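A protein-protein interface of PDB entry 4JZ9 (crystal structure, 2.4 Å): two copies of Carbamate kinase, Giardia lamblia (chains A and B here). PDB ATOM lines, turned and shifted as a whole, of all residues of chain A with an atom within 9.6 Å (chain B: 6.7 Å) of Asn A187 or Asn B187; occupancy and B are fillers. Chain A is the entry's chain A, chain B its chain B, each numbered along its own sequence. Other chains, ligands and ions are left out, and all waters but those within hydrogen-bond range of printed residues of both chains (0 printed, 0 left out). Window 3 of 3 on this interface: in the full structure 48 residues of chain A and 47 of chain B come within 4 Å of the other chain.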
ATOM      1  N   MET A   2      -9.655  34.073 -23.704  1.00  0.00           N
ATOM      2  CA  MET A   2     -10.523  35.212 -23.373  1.00  0.00           C
ATOM      3  C   MET A   2     -11.616  35.496 -24.435  1.00  0.00           C
ATOM      4  O   MET A   2     -11.388  35.355 -25.657  1.00  0.00           O
ATOM      5  CB  MET A   2      -9.681  36.463 -23.100  1.00  0.00           C
ATOM      6  CG  MET A   2      -8.766  36.849 -24.263  1.00  0.00           C
ATOM      7  SD  MET A   2      -9.233  38.415 -25.069  1.00  0.00           S
ATOM      8  CE  MET A   2      -7.834  38.683 -26.164  1.00  0.00           C
ATOM      9  N   SER A   3     -12.797  35.887 -23.951  1.00  0.00           N
ATOM     10  CA  SER A   3     -13.958  36.120 -24.807  1.00  0.00           C
ATOM     11  C   SER A   3     -13.666  36.992 -26.051  1.00  0.00           C
ATOM     12  O   SER A   3     -14.388  36.917 -27.051  1.00  0.00           O
ATOM     13  CB  SER A   3     -15.102  36.740 -23.981  1.00  0.00           C
ATOM     14  OG  SER A   3     -15.173  36.195 -22.665  1.00  0.00           O
ATOM     15  N   ALA A   4     -12.628  37.823 -25.996  1.00  0.00           N
ATOM     16  CA  ALA A   4     -12.401  38.788 -27.079  1.00  0.00           C
ATOM     17  C   ALA A   4     -11.571  38.267 -28.271  1.00  0.00           C
ATOM     18  O   ALA A   4     -11.651  38.817 -29.371  1.00  0.00           O
ATOM     19  CB  ALA A   4     -11.789  40.094 -26.531  1.00  0.00           C
ATOM     20  N   GLY A   5     -10.814  37.196 -28.056  1.00  0.00           N
ATOM     21  CA  GLY A   5      -9.791  36.765 -28.993  1.00  0.00           C
ATOM     22  C   GLY A   5     -10.244  36.089 -30.277  1.00  0.00           C
ATOM     23  O   GLY A   5     -11.219  35.335 -30.288  1.00  0.00           O
ATOM     24  N   THR A   7      -9.550  33.223 -33.102  1.00  0.00           N
ATOM     25  CA  THR A   7      -9.161  31.829 -32.949  1.00  0.00           C
ATOM     26  C   THR A   7      -8.061  31.424 -33.937  1.00  0.00           C
ATOM     27  O   THR A   7      -8.158  31.714 -35.135  1.00  0.00           O
ATOM     28  CB  THR A   7     -10.377  30.903 -33.113  1.00  0.00           C
ATOM     29  OG1 THR A   7     -11.311  31.196 -32.076  1.00  0.00           O
ATOM     30  CG2 THR A   7      -9.957  29.469 -33.004  1.00  0.00           C
ATOM     31  N   HIS A  44      -1.440  32.428 -26.332  1.00  0.00           N
ATOM     32  CA  HIS A  44      -2.624  32.470 -25.487  1.00  0.00           C
ATOM     33  C   HIS A  44      -2.550  33.692 -24.593  1.00  0.00           C
ATOM     34  O   HIS A  44      -3.560  34.342 -24.333  1.00  0.00           O
ATOM     35  CB  HIS A  44      -2.678  31.212 -24.610  1.00  0.00           C
ATOM     36  CG  HIS A  44      -3.566  31.348 -23.426  1.00  0.00           C
ATOM     37  ND1 HIS A  44      -4.932  31.147 -23.490  1.00  0.00           N
ATOM     38  CD2 HIS A  44      -3.298  31.683 -22.143  1.00  0.00           C
ATOM     39  CE1 HIS A  44      -5.458  31.353 -22.302  1.00  0.00           C
ATOM     40  NE2 HIS A  44      -4.483  31.683 -21.461  1.00  0.00           N
ATOM     41  N   LYS A  49      -7.469  32.654 -29.012  1.00  0.00           N
ATOM     42  CA  LYS A  49      -8.047  31.382 -28.588  1.00  0.00           C
ATOM     43  C   LYS A  49      -7.300  30.319 -29.375  1.00  0.00           C
ATOM     44  O   LYS A  49      -7.092  30.484 -30.582  1.00  0.00           O
ATOM     45  CB  LYS A  49      -9.553  31.266 -28.912  1.00  0.00           C
ATOM     46  CG  LYS A  49     -10.445  32.381 -28.446  1.00  0.00           C
ATOM     47  CD  LYS A  49     -11.600  31.839 -27.587  1.00  0.00           C
ATOM     48  CE  LYS A  49     -12.828  32.753 -27.566  1.00  0.00           C
ATOM     49  NZ  LYS A  49     -13.876  32.261 -28.508  1.00  0.00           N
ATOM     50  N   VAL A  50      -6.935  29.235 -28.701  1.00  0.00           N
ATOM     51  CA  VAL A  50      -6.141  28.160 -29.299  1.00  0.00           C
ATOM     52  C   VAL A  50      -6.807  26.773 -29.432  1.00  0.00           C
ATOM     53  O   VAL A  50      -7.305  26.178 -28.444  1.00  0.00           O
ATOM     54  CB  VAL A  50      -4.823  27.977 -28.526  1.00  0.00           C
ATOM     55  CG1 VAL A  50      -3.916  26.931 -29.226  1.00  0.00           C
ATOM     56  CG2 VAL A  50      -4.131  29.310 -28.400  1.00  0.00           C
ATOM     57  N   ASN A 110      -7.338  25.959 -17.804  1.00  0.00           N
ATOM     58  CA  ASN A 110      -8.378  25.252 -18.538  1.00  0.00           C
ATOM     59  C   ASN A 110      -7.964  24.903 -19.973  1.00  0.00           C
ATOM     60  O   ASN A 110      -7.960  25.736 -20.890  1.00  0.00           O
ATOM     61  CB  ASN A 110      -9.757  25.909 -18.459  1.00  0.00           C
ATOM     62  CG  ASN A 110      -9.860  27.066 -19.327  1.00  0.00           C
ATOM     63  OD1 ASN A 110      -8.904  27.829 -19.435  1.00  0.00           O
ATOM     64  ND2 ASN A 110     -10.991  27.209 -20.013  1.00  0.00           N
ATOM     65  N   CYS A 111      -7.605  23.635 -20.118  1.00  0.00           N
ATOM     66  CA  CYS A 111      -7.224  23.054 -21.376  1.00  0.00           C
ATOM     67  C   CYS A 111      -7.575  21.573 -21.279  1.00  0.00           C
ATOM     68  O   CYS A 111      -7.375  20.969 -20.236  1.00  0.00           O
ATOM     69  CB  CYS A 111      -5.723  23.293 -21.576  1.00  0.00           C
ATOM     70  SG  CYS A 111      -4.719  21.877 -22.047  1.00  0.00           S
ATOM     71  N   GLY A 179     -18.452  19.724 -33.417  1.00  0.00           N
ATOM     72  CA  GLY A 179     -19.468  20.377 -32.595  1.00  0.00           C
ATOM     73  C   GLY A 179     -19.055  20.565 -31.147  1.00  0.00           C
ATOM     74  O   GLY A 179     -19.252  21.623 -30.572  1.00  0.00           O
ATOM     75  N   VAL A 180     -18.452  19.546 -30.552  1.00  0.00           N
ATOM     76  CA  VAL A 180     -18.005  19.692 -29.188  1.00  0.00           C
ATOM     77  C   VAL A 180     -16.761  20.598 -29.076  1.00  0.00           C
ATOM     78  O   VAL A 180     -16.612  21.354 -28.101  1.00  0.00           O
ATOM     79  CB  VAL A 180     -17.779  18.303 -28.551  1.00  0.00           C
ATOM     80  CG1 VAL A 180     -17.258  18.441 -27.111  1.00  0.00           C
ATOM     81  CG2 VAL A 180     -19.089  17.461 -28.620  1.00  0.00           C
ATOM     82  N   ILE A 181     -15.873  20.527 -30.076  1.00  0.00           N
ATOM     83  CA  ILE A 181     -14.667  21.358 -30.071  1.00  0.00           C
ATOM     84  C   ILE A 181     -15.066  22.828 -30.180  1.00  0.00           C
ATOM     85  O   ILE A 181     -14.571  23.681 -29.437  1.00  0.00           O
ATOM     86  CB  ILE A 181     -13.622  20.958 -31.195  1.00  0.00           C
ATOM     87  CG1 ILE A 181     -13.117  19.540 -30.996  1.00  0.00           C
ATOM     88  CG2 ILE A 181     -12.400  21.837 -31.134  1.00  0.00           C
ATOM     89  CD1 ILE A 181     -12.948  18.747 -32.283  1.00  0.00           C
ATOM     90  N   LYS A 182     -15.989  23.123 -31.084  1.00  0.00           N
ATOM     91  CA  LYS A 182     -16.424  24.497 -31.243  1.00  0.00           C
ATOM     92  C   LYS A 182     -16.978  25.004 -29.936  1.00  0.00           C
ATOM     93  O   LYS A 182     -16.597  26.079 -29.465  1.00  0.00           O
ATOM     94  CB  LYS A 182     -17.480  24.604 -32.338  1.00  0.00           C
ATOM     95  CG  LYS A 182     -18.083  25.988 -32.476  1.00  0.00           C
ATOM     96  CD  LYS A 182     -18.797  26.100 -33.808  1.00  0.00           C
ATOM     97  CE  LYS A 182     -19.771  27.265 -33.837  1.00  0.00           C
ATOM     98  NZ  LYS A 182     -20.657  27.181 -35.048  1.00  0.00           N
ATOM     99  N   THR A 183     -17.884  24.223 -29.346  1.00  0.00           N
ATOM    100  CA  THR A 183     -18.432  24.542 -28.029  1.00  0.00           C
ATOM    101  C   THR A 183     -17.336  24.860 -26.991  1.00  0.00           C
ATOM    102  O   THR A 183     -17.443  25.810 -26.248  1.00  0.00           O
ATOM    103  CB  THR A 183     -19.254  23.393 -27.490  1.00  0.00           C
ATOM    104  OG1 THR A 183     -20.405  23.192 -28.319  1.00  0.00           O
ATOM    105  CG2 THR A 183     -19.682  23.703 -26.087  1.00  0.00           C
ATOM    106  N   LEU A 184     -16.278  24.056 -26.932  1.00  0.00           N
ATOM    107  CA  LEU A 184     -15.186  24.337 -26.002  1.00  0.00           C
ATOM    108  C   LEU A 184     -14.467  25.677 -26.258  1.00  0.00           C
ATOM    109  O   LEU A 184     -14.141  26.388 -25.308  1.00  0.00           O
ATOM    110  CB  LEU A 184     -14.172  23.190 -26.006  1.00  0.00           C
ATOM    111  CG  LEU A 184     -14.658  21.858 -25.420  1.00  0.00           C
ATOM    112  CD1 LEU A 184     -13.724  20.720 -25.810  1.00  0.00           C
ATOM    113  CD2 LEU A 184     -14.777  21.984 -23.905  1.00  0.00           C
ATOM    114  N   ILE A 185     -14.186  25.999 -27.525  1.00  0.00           N
ATOM    115  CA  ILE A 185     -13.478  27.243 -27.823  1.00  0.00           C
ATOM    116  C   ILE A 185     -14.388  28.434 -27.611  1.00  0.00           C
ATOM    117  O   ILE A 185     -13.966  29.416 -26.996  1.00  0.00           O
ATOM    118  CB  ILE A 185     -12.880  27.297 -29.231  1.00  0.00           C
ATOM    119  CG1 ILE A 185     -13.920  26.953 -30.283  1.00  0.00           C
ATOM    120  CG2 ILE A 185     -11.706  26.344 -29.344  1.00  0.00           C
ATOM    121  CD1 ILE A 185     -13.316  26.734 -31.650  1.00  0.00           C
ATOM    122  N   ASP A 186     -15.636  28.335 -28.079  1.00  0.00           N
ATOM    123  CA  ASP A 186     -16.651  29.311 -27.681  1.00  0.00           C
ATOM    124  C   ASP A 186     -16.502  29.717 -26.216  1.00  0.00           C
ATOM    125  O   ASP A 186     -16.775  30.865 -25.863  1.00  0.00           O
ATOM    126  CB  ASP A 186     -18.073  28.793 -27.889  1.00  0.00           C
ATOM    127  CG  ASP A 186     -18.489  28.771 -29.333  1.00  0.00           C
ATOM    128  OD1 ASP A 186     -17.717  29.267 -30.176  1.00  0.00           O
ATOM    129  OD2 ASP A 186     -19.604  28.270 -29.622  1.00  0.00           O
ATOM    130  N   ASN A 187     -16.081  28.784 -25.368  1.00  0.00           N
ATOM    131  CA  ASN A 187     -15.971  29.033 -23.932  1.00  0.00           C
ATOM    132  C   ASN A 187     -14.568  29.314 -23.495  1.00  0.00           C
ATOM    133  O   ASN A 187     -14.247  29.218 -22.320  1.00  0.00           O
ATOM    134  CB  ASN A 187     -16.503  27.853 -23.116  1.00  0.00           C
ATOM    135  CG  ASN A 187     -18.002  27.833 -23.057  1.00  0.00           C
ATOM    136  OD1 ASN A 187     -18.602  28.339 -22.103  1.00  0.00           O
ATOM    137  ND2 ASN A 187     -18.632  27.279 -24.089  1.00  0.00           N
ATOM    138  N   ASN A 188     -13.716  29.641 -24.449  1.00  0.00           N
ATOM    139  CA  ASN A 188     -12.363  30.036 -24.114  1.00  0.00           C
ATOM    140  C   ASN A 188     -11.537  28.904 -23.470  1.00  0.00           C
ATOM    141  O   ASN A 188     -10.660  29.170 -22.637  1.00  0.00           O
ATOM    142  CB  ASN A 188     -12.403  31.286 -23.211  1.00  0.00           C
ATOM    143  CG  ASN A 188     -13.611  32.215 -23.523  1.00  0.00           C
ATOM    144  OD1 ASN A 188     -13.870  32.564 -24.686  1.00  0.00           O
ATOM    145  ND2 ASN A 188     -14.359  32.599 -22.473  1.00  0.00           N
ATOM    146  N   VAL A 189     -11.822  27.652 -23.847  1.00  0.00           N
ATOM    147  CA  VAL A 189     -10.993  26.506 -23.429  1.00  0.00           C
ATOM    148  C   VAL A 189      -9.902  26.243 -24.466  1.00  0.00           C
ATOM    149  O   VAL A 189     -10.192  26.164 -25.664  1.00  0.00           O
ATOM    150  CB  VAL A 189     -11.817  25.173 -23.226  1.00  0.00           C
ATOM    151  CG1 VAL A 189     -10.947  24.078 -22.624  1.00  0.00           C
ATOM    152  CG2 VAL A 189     -13.046  25.415 -22.320  1.00  0.00           C
ATOM    153  N   LEU A 190      -8.653  26.108 -24.012  1.00  0.00           N
ATOM    154  CA  LEU A 190      -7.558  25.704 -24.905  1.00  0.00           C
ATOM    155  C   LEU A 190      -7.701  24.208 -25.228  1.00  0.00           C
ATOM    156  O   LEU A 190      -7.494  23.356 -24.367  1.00  0.00           O
ATOM    157  CB  LEU A 190      -6.197  26.043 -24.269  1.00  0.00           C
ATOM    158  CG  LEU A 190      -4.809  25.712 -24.870  1.00  0.00           C
ATOM    159  CD1 LEU A 190      -4.867  25.217 -26.287  1.00  0.00           C
ATOM    160  CD2 LEU A 190      -3.796  26.874 -24.754  1.00  0.00           C
ATOM    161  N   VAL A 191      -8.093  23.911 -26.467  1.00  0.00           N
ATOM    162  CA  VAL A 191      -8.435  22.549 -26.875  1.00  0.00           C
ATOM    163  C   VAL A 191      -7.311  21.784 -27.582  1.00  0.00           C
ATOM    164  O   VAL A 191      -6.756  22.260 -28.561  1.00  0.00           O
ATOM    165  CB  VAL A 191      -9.662  22.533 -27.830  1.00  0.00           C
ATOM    166  CG1 VAL A 191     -10.000  21.097 -28.256  1.00  0.00           C
ATOM    167  CG2 VAL A 191     -10.843  23.147 -27.179  1.00  0.00           C
ATOM    168  N   MET B   2     -29.584  18.522 -23.307  1.00  0.00           N
ATOM    169  CA  MET B   2     -30.767  19.377 -23.117  1.00  0.00           C
ATOM    170  C   MET B   2     -30.808  20.076 -21.733  1.00  0.00           C
ATOM    171  O   MET B   2     -30.575  19.450 -20.678  1.00  0.00           O
ATOM    172  CB  MET B   2     -32.059  18.600 -23.401  1.00  0.00           C
ATOM    173  CG  MET B   2     -33.141  19.443 -24.065  1.00  0.00           C
ATOM    174  SD  MET B   2     -34.701  19.461 -23.137  1.00  0.00           S
ATOM    175  CE  MET B   2     -34.140  19.972 -21.494  1.00  0.00           C
ATOM    176  N   LYS B  49     -28.473  14.694 -17.784  1.00  0.00           N
ATOM    177  CA  LYS B  49     -27.143  15.062 -18.236  1.00  0.00           C
ATOM    178  C   LYS B  49     -26.215  14.012 -17.706  1.00  0.00           C
ATOM    179  O   LYS B  49     -26.285  13.662 -16.523  1.00  0.00           O
ATOM    180  CB  LYS B  49     -26.728  16.435 -17.701  1.00  0.00           C
ATOM    181  CG  LYS B  49     -27.501  17.601 -18.311  1.00  0.00           C
ATOM    182  CD  LYS B  49     -26.986  18.959 -17.800  1.00  0.00           C
ATOM    183  CE  LYS B  49     -27.941  20.077 -18.195  1.00  0.00           C
ATOM    184  NZ  LYS B  49     -27.330  21.437 -18.086  1.00  0.00           N
ATOM    185  N   ASN B 110     -23.413  14.523 -29.920  1.00  0.00           N
ATOM    186  CA  ASN B 110     -22.441  15.312 -29.176  1.00  0.00           C
ATOM    187  C   ASN B 110     -22.053  14.660 -27.856  1.00  0.00           C
ATOM    188  O   ASN B 110     -22.705  14.783 -26.812  1.00  0.00           O
ATOM    189  CB  ASN B 110     -22.737  16.822 -29.097  1.00  0.00           C
ATOM    190  CG  ASN B 110     -23.754  17.170 -28.066  1.00  0.00           C
ATOM    191  OD1 ASN B 110     -24.743  16.452 -27.888  1.00  0.00           O
ATOM    192  ND2 ASN B 110     -23.533  18.288 -27.374  1.00  0.00           N
ATOM    193  N   LYS B 182     -17.160  20.413 -16.270  1.00  0.00           N
ATOM    194  CA  LYS B 182     -18.373  21.150 -15.943  1.00  0.00           C
ATOM    195  C   LYS B 182     -18.899  21.957 -17.123  1.00  0.00           C
ATOM    196  O   LYS B 182     -20.068  21.835 -17.502  1.00  0.00           O
ATOM    197  CB  LYS B 182     -18.220  22.069 -14.721  1.00  0.00           C
ATOM    198  CG  LYS B 182     -19.561  22.745 -14.417  1.00  0.00           C
ATOM    199  CD  LYS B 182     -19.718  23.271 -12.997  1.00  0.00           C
ATOM    200  CE  LYS B 182     -19.103  24.674 -12.826  1.00  0.00           C
ATOM    201  NZ  LYS B 182     -17.605  24.636 -12.805  1.00  0.00           N
ATOM    202  N   THR B 183     -18.040  22.801 -17.674  1.00  0.00           N
ATOM    203  CA  THR B 183     -18.379  23.580 -18.859  1.00  0.00           C
ATOM    204  C   THR B 183     -19.101  22.736 -19.914  1.00  0.00           C
ATOM    205  O   THR B 183     -20.098  23.145 -20.454  1.00  0.00           O
ATOM    206  CB  THR B 183     -17.098  24.176 -19.481  1.00  0.00           C
ATOM    207  OG1 THR B 183     -16.543  25.144 -18.589  1.00  0.00           O
ATOM    208  CG2 THR B 183     -17.366  24.809 -20.848  1.00  0.00           C
ATOM    209  N   LEU B 184     -18.589  21.546 -20.199  1.00  0.00           N
ATOM    210  CA  LEU B 184     -19.190  20.678 -21.202  1.00  0.00           C
ATOM    211  C   LEU B 184     -20.602  20.183 -20.825  1.00  0.00           C
ATOM    212  O   LEU B 184     -21.511  20.159 -21.657  1.00  0.00           O
ATOM    213  CB  LEU B 184     -18.262  19.501 -21.484  1.00  0.00           C
ATOM    214  CG  LEU B 184     -17.043  19.831 -22.353  1.00  0.00           C
ATOM    215  CD1 LEU B 184     -15.868  18.921 -22.008  1.00  0.00           C
ATOM    216  CD2 LEU B 184     -17.370  19.747 -23.845  1.00  0.00           C
ATOM    217  N   ILE B 185     -20.783  19.766 -19.579  1.00  0.00           N
ATOM    218  CA  ILE B 185     -22.101  19.347 -19.159  1.00  0.00           C
ATOM    219  C   ILE B 185     -23.058  20.538 -19.041  1.00  0.00           C
ATOM    220  O   ILE B 185     -24.249  20.402 -19.358  1.00  0.00           O
ATOM    221  CB  ILE B 185     -22.032  18.513 -17.873  1.00  0.00           C
ATOM    222  CG1 ILE B 185     -21.551  19.354 -16.697  1.00  0.00           C
ATOM    223  CG2 ILE B 185     -21.070  17.316 -18.100  1.00  0.00           C
ATOM    224  CD1 ILE B 185     -20.987  18.495 -15.544  1.00  0.00           C
ATOM    225  N   ASP B 186     -22.534  21.707 -18.642  1.00  0.00           N
ATOM    226  CA  ASP B 186     -23.340  22.930 -18.652  1.00  0.00           C
ATOM    227  C   ASP B 186     -23.854  23.183 -20.055  1.00  0.00           C
ATOM    228  O   ASP B 186     -24.912  23.755 -20.233  1.00  0.00           O
ATOM    229  CB  ASP B 186     -22.545  24.142 -18.185  1.00  0.00           C
ATOM    230  CG  ASP B 186     -22.408  24.229 -16.662  1.00  0.00           C
ATOM    231  OD1 ASP B 186     -22.738  23.265 -15.911  1.00  0.00           O
ATOM    232  OD2 ASP B 186     -21.936  25.296 -16.213  1.00  0.00           O
ATOM    233  N   ASN B 187     -23.095  22.756 -21.059  1.00  0.00           N
ATOM    234  CA  ASN B 187     -23.530  22.929 -22.437  1.00  0.00           C
ATOM    235  C   ASN B 187     -24.158  21.687 -22.986  1.00  0.00           C
ATOM    236  O   ASN B 187     -24.278  21.550 -24.204  1.00  0.00           O
ATOM    237  CB  ASN B 187     -22.389  23.360 -23.347  1.00  0.00           C
ATOM    238  CG  ASN B 187     -22.064  24.843 -23.222  1.00  0.00           C
ATOM    239  OD1 ASN B 187     -22.618  25.673 -23.955  1.00  0.00           O
ATOM    240  ND2 ASN B 187     -21.173  25.187 -22.290  1.00  0.00           N
ATOM    241  N   ASN B 188     -24.561  20.785 -22.087  1.00  0.00           N
ATOM    242  CA  ASN B 188     -25.290  19.577 -22.470  1.00  0.00           C
ATOM    243  C   ASN B 188     -24.494  18.630 -23.381  1.00  0.00           C
ATOM    244  O   ASN B 188     -25.007  18.103 -24.368  1.00  0.00           O
ATOM    245  CB  ASN B 188     -26.632  19.959 -23.110  1.00  0.00           C
ATOM    246  CG  ASN B 188     -27.314  21.145 -22.386  1.00  0.00           C
ATOM    247  OD1 ASN B 188     -27.681  21.025 -21.212  1.00  0.00           O
ATOM    248  ND2 ASN B 188     -27.476  22.291 -23.086  1.00  0.00           N
ATOM    249  N   VAL B 189     -23.222  18.434 -23.058  1.00  0.00           N
ATOM    250  CA  VAL B 189     -22.426  17.418 -23.748  1.00  0.00           C
ATOM    251  C   VAL B 189     -22.423  16.129 -22.916  1.00  0.00           C
ATOM    252  O   VAL B 189     -22.227  16.153 -21.692  1.00  0.00           O
ATOM    253  CB  VAL B 189     -20.996  17.924 -24.060  1.00  0.00           C
ATOM    254  CG1 VAL B 189     -20.161  16.891 -24.841  1.00  0.00           C
ATOM    255  CG2 VAL B 189     -21.080  19.233 -24.842  1.00  0.00           C
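Hydrophobic or aromatic side chains of chain B that line the printed part of chain A: Leu B184 and Val B189.
Of the 23 printed residues of chain A, 4 touch a printed residue of chain B.
Among the printed residues, 7 pairs touch across the chains.
Among the printed residues, no Asp or Glu carboxylate lies within 4 Å of a Lys or Arg side-chain nitrogen of the other chain.
Asn B110 touches Val A180 (CB to CG2, 3.7 Å).
CD2 of Leu B184 touches CG1 of Val A180, at 3.5 Å.
CG2 of Val A180 touches CG1 of Val B189, 3.97 Å away.
Asn B187 touches Thr A183 (CB to CG2, 3.9 Å).
Leu B184 touches Leu A184 (CD2 to CD2, 3.4 Å).
Asn A187 touches Thr B183 (CG to CG2, 3.8 Å).
ND2 of Asn A187 touches ND2 of Asn B187, at 3.8 Å.
Thr A183 touches Asn B187, and with the chains exchanged Asn A187 touches Thr B183.
Leu B184 touches its own counterpart, Leu A184.
Asn A187 touches its own counterpart, Asn B187.
Positions printed for both chains: 2, 49, 110, 182, 183, 184, 185, 186, 187, 188 and 189.
Asn A187 touches just these residues of chain B: Thr B183 (3.8 Å) and Asn B187 (3.8 Å).
Asn B187 touches just these residues of chain A: Thr A183 and Asn A187.
No residue of chain A comes within 4 Å of Asn B188.
Printed residues of chain A within 4 Å of Asn B110: Val A180.
Printed residues of chain A within 4 Å of Leu B184: Val A180 (3.5 Å) and Leu A184 (3.4 Å).
Printed residues of chain B within 4 Å of Leu A184: Leu B184.
The nearest residue of chain A that does not touch Asn B187 is Asp A186 (6.8 Å).
The nearest printed residue of chain A that does not touch Val B189 is Thr A183 (4.8 Å).
The side-chain amide nitrogen (ND2) of Asn B187 lies within hydrogen-bond range of the backbone carbonyl oxygen (O) of Thr B183 (2.9 Å).
The side-chain hydroxyl (OG1) of Thr A183 is in hydrogen-bond range of the backbone carbonyl oxygen (O) of Gly A179 (3.0 Å).
The side-chain amide nitrogen (ND2) of Asn B110 lies within hydrogen-bond range of the backbone carbonyl oxygen (O) of Asn B188, 3.4 Å away.
O of Thr A183 is in hydrogen-bond range of ND2 of Asn A187 (2.9 Å).
N of Val B189 sits at hydrogen-bond distance from O of Leu B184 (2.8 Å).
The backbone NH of Val A189 is in hydrogen-bond range of the backbone carbonyl oxygen of Leu A184, 3.0 Å away.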
